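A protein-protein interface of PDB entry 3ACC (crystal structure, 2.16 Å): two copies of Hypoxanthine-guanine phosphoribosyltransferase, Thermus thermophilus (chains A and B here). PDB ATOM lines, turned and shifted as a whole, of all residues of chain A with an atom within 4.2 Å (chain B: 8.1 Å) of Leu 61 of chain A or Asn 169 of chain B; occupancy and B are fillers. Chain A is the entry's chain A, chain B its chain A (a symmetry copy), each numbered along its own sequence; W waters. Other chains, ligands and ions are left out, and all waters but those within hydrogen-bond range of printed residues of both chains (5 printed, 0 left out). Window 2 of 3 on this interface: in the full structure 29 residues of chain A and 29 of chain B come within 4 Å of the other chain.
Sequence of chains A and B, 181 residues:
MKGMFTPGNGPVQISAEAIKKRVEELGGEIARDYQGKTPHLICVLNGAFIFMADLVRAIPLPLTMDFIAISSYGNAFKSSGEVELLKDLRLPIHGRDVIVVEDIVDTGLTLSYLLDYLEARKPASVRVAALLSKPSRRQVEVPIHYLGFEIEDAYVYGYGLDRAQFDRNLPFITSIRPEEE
Water W1 lies within hydrogen-bond range of the backbone carbonyl oxygen (O) of Gln 165 of chain B (2.6 Å), the guanidinium group (NE) of Arg 168 of chain B (2.9 Å) and the backbone NH (N) of Met 65 of chain A (3.1 Å).
Water W4 lies within hydrogen-bond range of O of Met 65 of chain A, OE1 of Gln 165 of chain B and NH2 of Arg 168 of chain B.
Water W5 lies within hydrogen-bond range of OD1 of Asn 169 of chain B (2.7 Å), N of Asp 167 of chain B (2.8 Å) and N of Leu 63 of chain A (3.0 Å).
Water W2 bridges O of Pro 171 of chain B (2.7 Å) and NH1 of Arg 57 of chain A (3.1 Å).
Water W3 lies within hydrogen-bond range of O of Leu 63 of chain A (2.8 Å), O of Gln 165 of chain B (2.8 Å), N of Arg 168 of chain B (3.0 Å) and N of Asp 167 of chain B (3.3 Å).
No position is printed for both chains.
Of the 16 pairs that touch across the chains among the printed residues, none has its exchanged pair printed and touching as well.
CE2 of Phe 5 of chain B touches O of Arg 57 of chain A, 3.4 Å away.
CG2 of Ile 50 of chain B touches NH1 of Arg 57 of chain A (3.5 Å).
Asn 169 of chain B touches Arg 57 of chain A.
Ile 59 of chain A touches Phe 5 of chain B.
CA of Pro 60 of chain A touches CZ of Phe 5 of chain B, 3.7 Å away.
Gln 165 of chain B touches Leu 63 of chain A (O to O, 3.8 Å).
Phe 166 of chain B touches Leu 63 of chain A.
Leu 63 of chain A touches Asn 169 of chain B.
Met 65 of chain A touches Phe 49 of chain B.
Met 65 of chain A touches Asn 169 of chain B (CE to N, 3.9 Å).
The backbone NH of Tyr 159 of chain B is in hydrogen-bond range of the backbone carbonyl oxygen of Leu 170 of chain B (2.7 Å).
The backbone NH (N) of Gly 160 of chain B sits at hydrogen-bond distance from the backbone carbonyl oxygen (O) of Arg 168 of chain B (2.8 Å).
OD2 of Asp 162 of chain B lies within hydrogen-bond range of N of Gln 165 of chain B, 2.8 Å away.
The guanidinium group (NH1) of Arg 168 of chain B lies within salt-bridge range of the side-chain carboxylate (OD1) of Asp 162 of chain B (3.5 Å).
OE1 of Gln 165 of chain B lies within hydrogen-bond range of NH2 of Arg 168 of chain B, at 3.2 Å.
Of chain B, only Asn 169 comes within 4 Å of Leu 61 of chain A.
No residue of chain B comes within 4 Å of Pro 62 of chain A.
Of the printed residues of chain A, Phe 166 of chain B touches Leu 63.
Of the printed residues of chain A, Gly 3 of chain B touches Pro 60 (3.5 Å).
Printed residues of chain B within 4 Å of Val 56 of chain A: Asn 169 (3.2 Å).
Leu 161 of chain B touches none of the printed residues of chain A.
Asp 167 of chain B touches none of the printed residues of chain A.
The nearest printed residue of chain A that does not touch Asn 169 of chain B is Pro 60 of chain A (4.9 Å).
Of the 11 printed residues of chain A, 7 touch a printed residue of chain B.
Printed residues of chain A that touch a printed residue of chain B: Val 56, Arg 57, Ile 59, Pro 60, Leu 61, Leu 63 and Met 65.
Hydrophobic or aromatic side chains of chain A that line the printed part of chain B: Val 56, Pro 60, Leu 63 and Met 65.
Hydrophobic or aromatic side chains of chain B that line the printed part of chain A: Phe 5, Phe 49, Ile 50, Tyr 159 and Phe 166.
Along chain B the printed residues that touch a printed residue of chain A span positions 3 to 169.
Among the printed residues, 16 pairs touch across the chains.
Among the printed residues, no Asp or Glu carboxylate lies within 4 Å of a Lys or Arg side-chain nitrogen of the other chain.
O of Ile 59 of chain A lies within hydrogen-bond range of ND2 of Asn 169 of chain B.
ND2 of Asn 169 of chain B sits at hydrogen-bond distance from O of Leu 61 of chain A, 3.1 Å away.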
ATOM      1  N   ALA A  31     -11.598   3.524 -34.370  1.00  0.00           N
ATOM      2  CA  ALA A  31     -12.146   3.912 -33.076  1.00  0.00           C
ATOM      3  C   ALA A  31     -13.277   2.963 -32.684  1.00  0.00           C
ATOM      4  O   ALA A  31     -13.335   2.473 -31.553  1.00  0.00           O
ATOM      5  CB  ALA A  31     -12.653   5.352 -33.131  1.00  0.00           C
ATOM      6  N   TYR A  34     -11.891  -0.764 -32.123  1.00  0.00           N
ATOM      7  CA  TYR A  34     -11.029  -0.872 -30.945  1.00  0.00           C
ATOM      8  C   TYR A  34     -11.587  -0.252 -29.678  1.00  0.00           C
ATOM      9  O   TYR A  34     -10.844  -0.005 -28.722  1.00  0.00           O
ATOM     10  CB  TYR A  34      -9.662  -0.250 -31.247  1.00  0.00           C
ATOM     11  CG  TYR A  34      -8.814  -1.104 -32.154  1.00  0.00           C
ATOM     12  CD1 TYR A  34      -7.812  -1.921 -31.636  1.00  0.00           C
ATOM     13  CD2 TYR A  34      -9.048  -1.135 -33.529  1.00  0.00           C
ATOM     14  CE1 TYR A  34      -7.064  -2.755 -32.464  1.00  0.00           C
ATOM     15  CE2 TYR A  34      -8.309  -1.964 -34.368  1.00  0.00           C
ATOM     16  CZ  TYR A  34      -7.319  -2.773 -33.830  1.00  0.00           C
ATOM     17  OH  TYR A  34      -6.593  -3.602 -34.657  1.00  0.00           O
ATOM     18  N   GLN A  35     -12.891  -0.003 -29.662  1.00  0.00           N
ATOM     19  CA  GLN A  35     -13.518   0.586 -28.491  1.00  0.00           C
ATOM     20  C   GLN A  35     -13.198  -0.300 -27.289  1.00  0.00           C
ATOM     21  O   GLN A  35     -13.192  -1.529 -27.395  1.00  0.00           O
ATOM     22  CB  GLN A  35     -15.032   0.686 -28.697  1.00  0.00           C
ATOM     23  CG  GLN A  35     -15.689   1.802 -27.897  1.00  0.00           C
ATOM     24  CD  GLN A  35     -15.115   3.172 -28.233  1.00  0.00           C
ATOM     25  OE1 GLN A  35     -15.200   3.635 -29.374  1.00  0.00           O
ATOM     26  NE2 GLN A  35     -14.525   3.825 -27.234  1.00  0.00           N
ATOM     27  N   VAL A  56      -4.075   9.269 -36.746  1.00  0.00           N
ATOM     28  CA  VAL A  56      -4.153   9.250 -35.289  1.00  0.00           C
ATOM     29  C   VAL A  56      -5.052  10.347 -34.725  1.00  0.00           C
ATOM     30  O   VAL A  56      -5.707  10.156 -33.697  1.00  0.00           O
ATOM     31  CB  VAL A  56      -2.751   9.365 -34.646  1.00  0.00           C
ATOM     32  CG1 VAL A  56      -1.866   8.207 -35.122  1.00  0.00           C
ATOM     33  CG2 VAL A  56      -2.121  10.718 -34.986  1.00  0.00           C
ATOM     34  N   ARG A  57      -5.090  11.491 -35.398  1.00  0.00           N
ATOM     35  CA  ARG A  57      -5.920  12.600 -34.948  1.00  0.00           C
ATOM     36  C   ARG A  57      -7.396  12.339 -35.228  1.00  0.00           C
ATOM     37  O   ARG A  57      -8.260  13.127 -34.840  1.00  0.00           O
ATOM     38  CB  ARG A  57      -5.466  13.897 -35.621  1.00  0.00           C
ATOM     39  CG  ARG A  57      -4.158  14.436 -35.050  1.00  0.00           C
ATOM     40  CD  ARG A  57      -3.738  15.730 -35.710  1.00  0.00           C
ATOM     41  NE  ARG A  57      -3.183  15.532 -37.044  1.00  0.00           N
ATOM     42  CZ  ARG A  57      -2.689  16.519 -37.783  1.00  0.00           C
ATOM     43  NH1 ARG A  57      -2.692  17.752 -37.305  1.00  0.00           N
ATOM     44  NH2 ARG A  57      -2.190  16.275 -38.991  1.00  0.00           N
ATOM     45  N   ILE A  59      -8.683   9.249 -34.416  1.00  0.00           N
ATOM     46  CA  ILE A  59      -8.956   8.075 -33.595  1.00  0.00           C
ATOM     47  C   ILE A  59      -9.071   8.508 -32.137  1.00  0.00           C
ATOM     48  O   ILE A  59      -8.069   8.570 -31.417  1.00  0.00           O
ATOM     49  CB  ILE A  59      -7.828   7.027 -33.697  1.00  0.00           C
ATOM     50  CG1 ILE A  59      -7.669   6.563 -35.143  1.00  0.00           C
ATOM     51  CG2 ILE A  59      -8.143   5.839 -32.799  1.00  0.00           C
ATOM     52  CD1 ILE A  59      -6.516   5.592 -35.344  1.00  0.00           C
ATOM     53  N   PRO A  60     -10.298   8.813 -31.684  1.00  0.00           N
ATOM     54  CA  PRO A  60     -10.609   9.250 -30.316  1.00  0.00           C
ATOM     55  C   PRO A  60     -10.463   8.154 -29.262  1.00  0.00           C
ATOM     56  O   PRO A  60     -11.422   7.842 -28.558  1.00  0.00           O
ATOM     57  CB  PRO A  60     -12.062   9.726 -30.422  1.00  0.00           C
ATOM     58  CG  PRO A  60     -12.225  10.067 -31.874  1.00  0.00           C
ATOM     59  CD  PRO A  60     -11.483   8.947 -32.548  1.00  0.00           C
ATOM     60  N   LEU A  61      -9.269   7.579 -29.152  1.00  0.00           N
ATOM     61  CA  LEU A  61      -9.008   6.518 -28.181  1.00  0.00           C
ATOM     62  C   LEU A  61      -7.651   6.702 -27.516  1.00  0.00           C
ATOM     63  O   LEU A  61      -6.775   7.371 -28.053  1.00  0.00           O
ATOM     64  CB  LEU A  61      -8.986   5.145 -28.866  1.00  0.00           C
ATOM     65  CG  LEU A  61     -10.234   4.507 -29.466  1.00  0.00           C
ATOM     66  CD1 LEU A  61      -9.827   3.203 -30.141  1.00  0.00           C
ATOM     67  CD2 LEU A  61     -11.275   4.248 -28.375  1.00  0.00           C
ATOM     68  N   PRO A  62      -7.465   6.116 -26.323  1.00  0.00           N
ATOM     69  CA  PRO A  62      -6.160   6.260 -25.674  1.00  0.00           C
ATOM     70  C   PRO A  62      -5.266   5.287 -26.442  1.00  0.00           C
ATOM     71  O   PRO A  62      -5.629   4.124 -26.632  1.00  0.00           O
ATOM     72  CB  PRO A  62      -6.434   5.804 -24.246  1.00  0.00           C
ATOM     73  CG  PRO A  62      -7.488   4.730 -24.444  1.00  0.00           C
ATOM     74  CD  PRO A  62      -8.409   5.369 -25.471  1.00  0.00           C
ATOM     75  N   LEU A  63      -4.122   5.756 -26.916  1.00  0.00           N
ATOM     76  CA  LEU A  63      -3.242   4.883 -27.678  1.00  0.00           C
ATOM     77  C   LEU A  63      -1.796   5.333 -27.602  1.00  0.00           C
ATOM     78  O   LEU A  63      -1.501   6.439 -27.139  1.00  0.00           O
ATOM     79  CB  LEU A  63      -3.702   4.841 -29.143  1.00  0.00           C
ATOM     80  CG  LEU A  63      -3.777   6.172 -29.898  1.00  0.00           C
ATOM     81  CD1 LEU A  63      -2.405   6.530 -30.469  1.00  0.00           C
ATOM     82  CD2 LEU A  63      -4.794   6.060 -31.036  1.00  0.00           C
ATOM     83  N   MET A  65       2.247   4.967 -29.736  1.00  0.00           N
ATOM     84  CA  MET A  65       2.784   4.772 -31.069  1.00  0.00           C
ATOM     85  C   MET A  65       4.280   4.596 -31.094  1.00  0.00           C
ATOM     86  O   MET A  65       4.968   4.872 -30.116  1.00  0.00           O
ATOM     87  CB  MET A  65       2.366   5.929 -31.993  1.00  0.00           C
ATOM     88  CG  MET A  65       1.988   7.230 -31.301  1.00  0.00           C
ATOM     89  SD  MET A  65       1.420   8.509 -32.471  1.00  0.00           S
ATOM     90  CE  MET A  65      -0.210   8.877 -31.852  1.00  0.00           C
ATOM     91  N   GLY B   3     -15.990   8.138 -26.262  1.00  0.00           N
ATOM     92  CA  GLY B   3     -14.598   8.459 -26.692  1.00  0.00           C
ATOM     93  C   GLY B   3     -14.489   9.812 -27.369  1.00  0.00           C
ATOM     94  O   GLY B   3     -14.946   9.991 -28.498  1.00  0.00           O
ATOM     95  N   MET B   4     -13.885  10.773 -26.674  1.00  0.00           N
ATOM     96  CA  MET B   4     -13.714  12.118 -27.214  1.00  0.00           C
ATOM     97  C   MET B   4     -12.409  12.731 -26.727  1.00  0.00           C
ATOM     98  O   MET B   4     -11.919  12.389 -25.653  1.00  0.00           O
ATOM     99  CB  MET B   4     -14.878  13.019 -26.790  1.00  0.00           C
ATOM    100  CG  MET B   4     -16.238  12.595 -27.318  1.00  0.00           C
ATOM    101  SD  MET B   4     -17.543  13.762 -26.863  1.00  0.00           S
ATOM    102  CE  MET B   4     -18.053  13.102 -25.274  1.00  0.00           C
ATOM    103  N   PHE B   5     -11.849  13.636 -27.524  1.00  0.00           N
ATOM    104  CA  PHE B   5     -10.610  14.307 -27.157  1.00  0.00           C
ATOM    105  C   PHE B   5     -10.922  15.338 -26.081  1.00  0.00           C
ATOM    106  O   PHE B   5     -11.751  16.225 -26.281  1.00  0.00           O
ATOM    107  CB  PHE B   5      -9.988  14.986 -28.383  1.00  0.00           C
ATOM    108  CG  PHE B   5      -9.518  14.018 -29.439  1.00  0.00           C
ATOM    109  CD1 PHE B   5      -8.611  13.012 -29.121  1.00  0.00           C
ATOM    110  CD2 PHE B   5      -9.974  14.117 -30.752  1.00  0.00           C
ATOM    111  CE1 PHE B   5      -8.162  12.116 -30.092  1.00  0.00           C
ATOM    112  CE2 PHE B   5      -9.531  13.227 -31.730  1.00  0.00           C
ATOM    113  CZ  PHE B   5      -8.623  12.226 -31.399  1.00  0.00           C
ATOM    114  N   PHE B  49       6.626  14.752 -35.245  1.00  0.00           N
ATOM    115  CA  PHE B  49       6.121  14.183 -36.491  1.00  0.00           C
ATOM    116  C   PHE B  49       4.796  14.749 -37.020  1.00  0.00           C
ATOM    117  O   PHE B  49       4.566  14.725 -38.228  1.00  0.00           O
ATOM    118  CB  PHE B  49       6.054  12.651 -36.386  1.00  0.00           C
ATOM    119  CG  PHE B  49       4.740  12.118 -35.890  1.00  0.00           C
ATOM    120  CD1 PHE B  49       3.778  11.666 -36.788  1.00  0.00           C
ATOM    121  CD2 PHE B  49       4.481  12.028 -34.529  1.00  0.00           C
ATOM    122  CE1 PHE B  49       2.575  11.126 -36.331  1.00  0.00           C
ATOM    123  CE2 PHE B  49       3.282  11.489 -34.064  1.00  0.00           C
ATOM    124  CZ  PHE B  49       2.330  11.037 -34.969  1.00  0.00           C
ATOM    125  N   ILE B  50       3.929  15.250 -36.142  1.00  0.00           N
ATOM    126  CA  ILE B  50       2.672  15.822 -36.608  1.00  0.00           C
ATOM    127  C   ILE B  50       2.947  17.253 -37.063  1.00  0.00           C
ATOM    128  O   ILE B  50       2.449  17.696 -38.100  1.00  0.00           O
ATOM    129  CB  ILE B  50       1.578  15.810 -35.508  1.00  0.00           C
ATOM    130  CG1 ILE B  50       1.215  14.356 -35.162  1.00  0.00           C
ATOM    131  CG2 ILE B  50       0.342  16.571 -35.995  1.00  0.00           C
ATOM    132  CD1 ILE B  50       0.012  14.196 -34.248  1.00  0.00           C
ATOM    133  N   TYR B 157       1.145  18.550 -23.862  1.00  0.00           N
ATOM    134  CA  TYR B 157       1.049  17.290 -24.579  1.00  0.00           C
ATOM    135  C   TYR B 157      -0.025  17.424 -25.645  1.00  0.00           C
ATOM    136  O   TYR B 157      -0.803  18.383 -25.634  1.00  0.00           O
ATOM    137  CB  TYR B 157       0.753  16.129 -23.620  1.00  0.00           C
ATOM    138  CG  TYR B 157      -0.547  16.224 -22.850  1.00  0.00           C
ATOM    139  CD1 TYR B 157      -1.715  15.637 -23.341  1.00  0.00           C
ATOM    140  CD2 TYR B 157      -0.601  16.869 -21.613  1.00  0.00           C
ATOM    141  CE1 TYR B 157      -2.900  15.683 -22.614  1.00  0.00           C
ATOM    142  CE2 TYR B 157      -1.789  16.925 -20.878  1.00  0.00           C
ATOM    143  CZ  TYR B 157      -2.933  16.327 -21.383  1.00  0.00           C
ATOM    144  OH  TYR B 157      -4.105  16.369 -20.662  1.00  0.00           O
ATOM    145  N   GLY B 158      -0.050  16.477 -26.575  1.00  0.00           N
ATOM    146  CA  GLY B 158      -1.013  16.527 -27.655  1.00  0.00           C
ATOM    147  C   GLY B 158      -0.305  16.975 -28.920  1.00  0.00           C
ATOM    148  O   GLY B 158       0.842  17.426 -28.863  1.00  0.00           O
ATOM    149  N   TYR B 159      -0.975  16.839 -30.058  1.00  0.00           N
ATOM    150  CA  TYR B 159      -0.419  17.237 -31.349  1.00  0.00           C
ATOM    151  C   TYR B 159       0.987  16.649 -31.559  1.00  0.00           C
ATOM    152  O   TYR B 159       1.910  17.343 -32.007  1.00  0.00           O
ATOM    153  CB  TYR B 159      -0.378  18.772 -31.447  1.00  0.00           C
ATOM    154  CG  TYR B 159      -0.148  19.309 -32.848  1.00  0.00           C
ATOM    155  CD1 TYR B 159      -1.158  19.265 -33.812  1.00  0.00           C
ATOM    156  CD2 TYR B 159       1.083  19.844 -33.214  1.00  0.00           C
ATOM    157  CE1 TYR B 159      -0.943  19.747 -35.116  1.00  0.00           C
ATOM    158  CE2 TYR B 159       1.315  20.319 -34.512  1.00  0.00           C
ATOM    159  CZ  TYR B 159       0.300  20.267 -35.457  1.00  0.00           C
ATOM    160  OH  TYR B 159       0.547  20.705 -36.747  1.00  0.00           O
ATOM    161  N   GLY B 160       1.141  15.367 -31.233  1.00  0.00           N
ATOM    162  CA  GLY B 160       2.429  14.711 -31.389  1.00  0.00           C
ATOM    163  C   GLY B 160       3.196  14.540 -30.084  1.00  0.00           C
ATOM    164  O   GLY B 160       3.934  13.568 -29.917  1.00  0.00           O
ATOM    165  N   LEU B 161       3.027  15.483 -29.161  1.00  0.00           N
ATOM    166  CA  LEU B 161       3.712  15.423 -27.875  1.00  0.00           C
ATOM    167  C   LEU B 161       2.970  14.484 -26.930  1.00  0.00           C
ATOM    168  O   LEU B 161       1.741  14.476 -26.869  1.00  0.00           O
ATOM    169  CB  LEU B 161       3.838  16.822 -27.262  1.00  0.00           C
ATOM    170  CG  LEU B 161       4.760  17.798 -28.009  1.00  0.00           C
ATOM    171  CD1 LEU B 161       4.145  18.184 -29.354  1.00  0.00           C
ATOM    172  CD2 LEU B 161       4.981  19.042 -27.167  1.00  0.00           C
ATOM    173  N   ASP B 162       3.729  13.701 -26.177  1.00  0.00           N
ATOM    174  CA  ASP B 162       3.143  12.716 -25.288  1.00  0.00           C
ATOM    175  C   ASP B 162       3.083  13.053 -23.809  1.00  0.00           C
ATOM    176  O   ASP B 162       3.675  14.024 -23.320  1.00  0.00           O
ATOM    177  CB  ASP B 162       3.907  11.401 -25.426  1.00  0.00           C
ATOM    178  CG  ASP B 162       5.273  11.465 -24.765  1.00  0.00           C
ATOM    179  OD1 ASP B 162       6.069  12.343 -25.147  1.00  0.00           O
ATOM    180  OD2 ASP B 162       5.548  10.650 -23.860  1.00  0.00           O
ATOM    181  N   GLN B 165       3.886   8.539 -23.120  1.00  0.00           N
ATOM    182  CA  GLN B 165       3.614   7.830 -24.372  1.00  0.00           C
ATOM    183  C   GLN B 165       2.179   7.937 -24.907  1.00  0.00           C
ATOM    184  O   GLN B 165       1.912   7.572 -26.054  1.00  0.00           O
ATOM    185  CB  GLN B 165       4.004   6.351 -24.242  1.00  0.00           C
ATOM    186  CG  GLN B 165       5.502   6.113 -24.062  1.00  0.00           C
ATOM    187  CD  GLN B 165       6.349   6.807 -25.127  1.00  0.00           C
ATOM    188  OE1 GLN B 165       5.952   6.905 -26.293  1.00  0.00           O
ATOM    189  NE2 GLN B 165       7.524   7.281 -24.731  1.00  0.00           N
ATOM    190  N   PHE B 166       1.266   8.443 -24.086  1.00  0.00           N
ATOM    191  CA  PHE B 166      -0.132   8.602 -24.481  1.00  0.00           C
ATOM    192  C   PHE B 166      -0.435  10.034 -24.928  1.00  0.00           C
ATOM    193  O   PHE B 166       0.382  10.937 -24.761  1.00  0.00           O
ATOM    194  CB  PHE B 166      -1.052   8.252 -23.304  1.00  0.00           C
ATOM    195  CG  PHE B 166      -1.185   6.781 -23.049  1.00  0.00           C
ATOM    196  CD1 PHE B 166      -2.045   6.001 -23.825  1.00  0.00           C
ATOM    197  CD2 PHE B 166      -0.443   6.165 -22.046  1.00  0.00           C
ATOM    198  CE1 PHE B 166      -2.162   4.634 -23.607  1.00  0.00           C
ATOM    199  CE2 PHE B 166      -0.555   4.791 -21.819  1.00  0.00           C
ATOM    200  CZ  PHE B 166      -1.414   4.027 -22.601  1.00  0.00           C
ATOM    201  N   ASP B 167      -1.614  10.223 -25.509  1.00  0.00           N
ATOM    202  CA  ASP B 167      -2.090  11.534 -25.944  1.00  0.00           C
ATOM    203  C   ASP B 167      -1.360  12.267 -27.069  1.00  0.00           C
ATOM    204  O   ASP B 167      -1.514  13.487 -27.210  1.00  0.00           O
ATOM    205  CB  ASP B 167      -2.193  12.468 -24.736  1.00  0.00           C
ATOM    206  CG  ASP B 167      -3.091  11.909 -23.647  1.00  0.00           C
ATOM    207  OD1 ASP B 167      -4.236  11.516 -23.957  1.00  0.00           O
ATOM    208  OD2 ASP B 167      -2.650  11.866 -22.479  1.00  0.00           O
ATOM    209  N   ARG B 168      -0.569  11.548 -27.860  1.00  0.00           N
ATOM    210  CA  ARG B 168       0.115  12.190 -28.981  1.00  0.00           C
ATOM    211  C   ARG B 168      -0.923  12.451 -30.074  1.00  0.00           C
ATOM    212  O   ARG B 168      -0.703  13.276 -30.957  1.00  0.00           O
ATOM    213  CB  ARG B 168       1.207  11.290 -29.574  1.00  0.00           C
ATOM    214  CG  ARG B 168       2.427  11.016 -28.698  1.00  0.00           C
ATOM    215  CD  ARG B 168       3.422  10.171 -29.505  1.00  0.00           C
ATOM    216  NE  ARG B 168       4.524   9.637 -28.709  1.00  0.00           N
ATOM    217  CZ  ARG B 168       5.552  10.357 -28.272  1.00  0.00           C
ATOM    218  NH1 ARG B 168       5.624  11.651 -28.551  1.00  0.00           N
ATOM    219  NH2 ARG B 168       6.513   9.778 -27.567  1.00  0.00           N
ATOM    220  N   ASN B 169      -2.055  11.744 -30.003  1.00  0.00           N
ATOM    221  CA  ASN B 169      -3.106  11.878 -31.010  1.00  0.00           C
ATOM    222  C   ASN B 169      -4.115  13.014 -30.832  1.00  0.00           C
ATOM    223  O   ASN B 169      -4.938  13.247 -31.716  1.00  0.00           O
ATOM    224  CB  ASN B 169      -3.841  10.537 -31.187  1.00  0.00           C
ATOM    225  CG  ASN B 169      -4.466  10.017 -29.898  1.00  0.00           C
ATOM    226  OD1 ASN B 169      -3.854  10.060 -28.829  1.00  0.00           O
ATOM    227  ND2 ASN B 169      -5.682   9.491 -30.006  1.00  0.00           N
ATOM    228  N   LEU B 170      -4.067  13.722 -29.708  1.00  0.00           N
ATOM    229  CA  LEU B 170      -4.981  14.850 -29.516  1.00  0.00           C
ATOM    230  C   LEU B 170      -4.653  15.867 -30.614  1.00  0.00           C
ATOM    231  O   LEU B 170      -3.490  16.216 -30.815  1.00  0.00           O
ATOM    232  CB  LEU B 170      -4.782  15.482 -28.137  1.00  0.00           C
ATOM    233  CG  LEU B 170      -5.613  14.944 -26.963  1.00  0.00           C
ATOM    234  CD1 LEU B 170      -5.511  13.427 -26.874  1.00  0.00           C
ATOM    235  CD2 LEU B 170      -5.126  15.599 -25.675  1.00  0.00           C
ATOM    236  N   PRO B 171      -5.673  16.348 -31.345  1.00  0.00           N
ATOM    237  CA  PRO B 171      -5.440  17.323 -32.418  1.00  0.00           C
ATOM    238  C   PRO B 171      -5.066  18.727 -31.942  1.00  0.00           C
ATOM    239  O   PRO B 171      -4.768  19.617 -32.745  1.00  0.00           O
ATOM    240  CB  PRO B 171      -6.753  17.296 -33.193  1.00  0.00           C
ATOM    241  CG  PRO B 171      -7.760  17.004 -32.132  1.00  0.00           C
ATOM    242  CD  PRO B 171      -7.086  15.932 -31.310  1.00  0.00           C
ATOM    243  N   PHE B 172      -5.068  18.916 -30.629  1.00  0.00           N
ATOM    244  CA  PHE B 172      -4.745  20.212 -30.048  1.00  0.00           C
ATOM    245  C   PHE B 172      -3.663  20.081 -28.989  1.00  0.00           C
ATOM    246  O   PHE B 172      -3.353  18.978 -28.540  1.00  0.00           O
ATOM    247  CB  PHE B 172      -6.004  20.812 -29.420  1.00  0.00           C
ATOM    248  CG  PHE B 172      -6.678  19.900 -28.432  1.00  0.00           C
ATOM    249  CD1 PHE B 172      -6.134  19.691 -27.166  1.00  0.00           C
ATOM    250  CD2 PHE B 172      -7.858  19.237 -28.771  1.00  0.00           C
ATOM    251  CE1 PHE B 172      -6.751  18.839 -26.254  1.00  0.00           C
ATOM    252  CE2 PHE B 172      -8.482  18.383 -27.866  1.00  0.00           C
ATOM    253  CZ  PHE B 172      -7.926  18.186 -26.603  1.00  0.00           C
HETATM  254  O   HOH W   1       3.595   7.049 -27.927  1.00  0.00           O
HETATM  255  O   HOH W   2      -4.571  19.228 -35.388  1.00  0.00           O
HETATM  256  O   HOH W   3       0.067   8.616 -27.899  1.00  0.00           O
HETATM  257  O   HOH W   4       6.513   6.563 -28.836  1.00  0.00           O
HETATM  258  O   HOH W   5      -3.725   8.703 -26.549  1.00  0.00           O
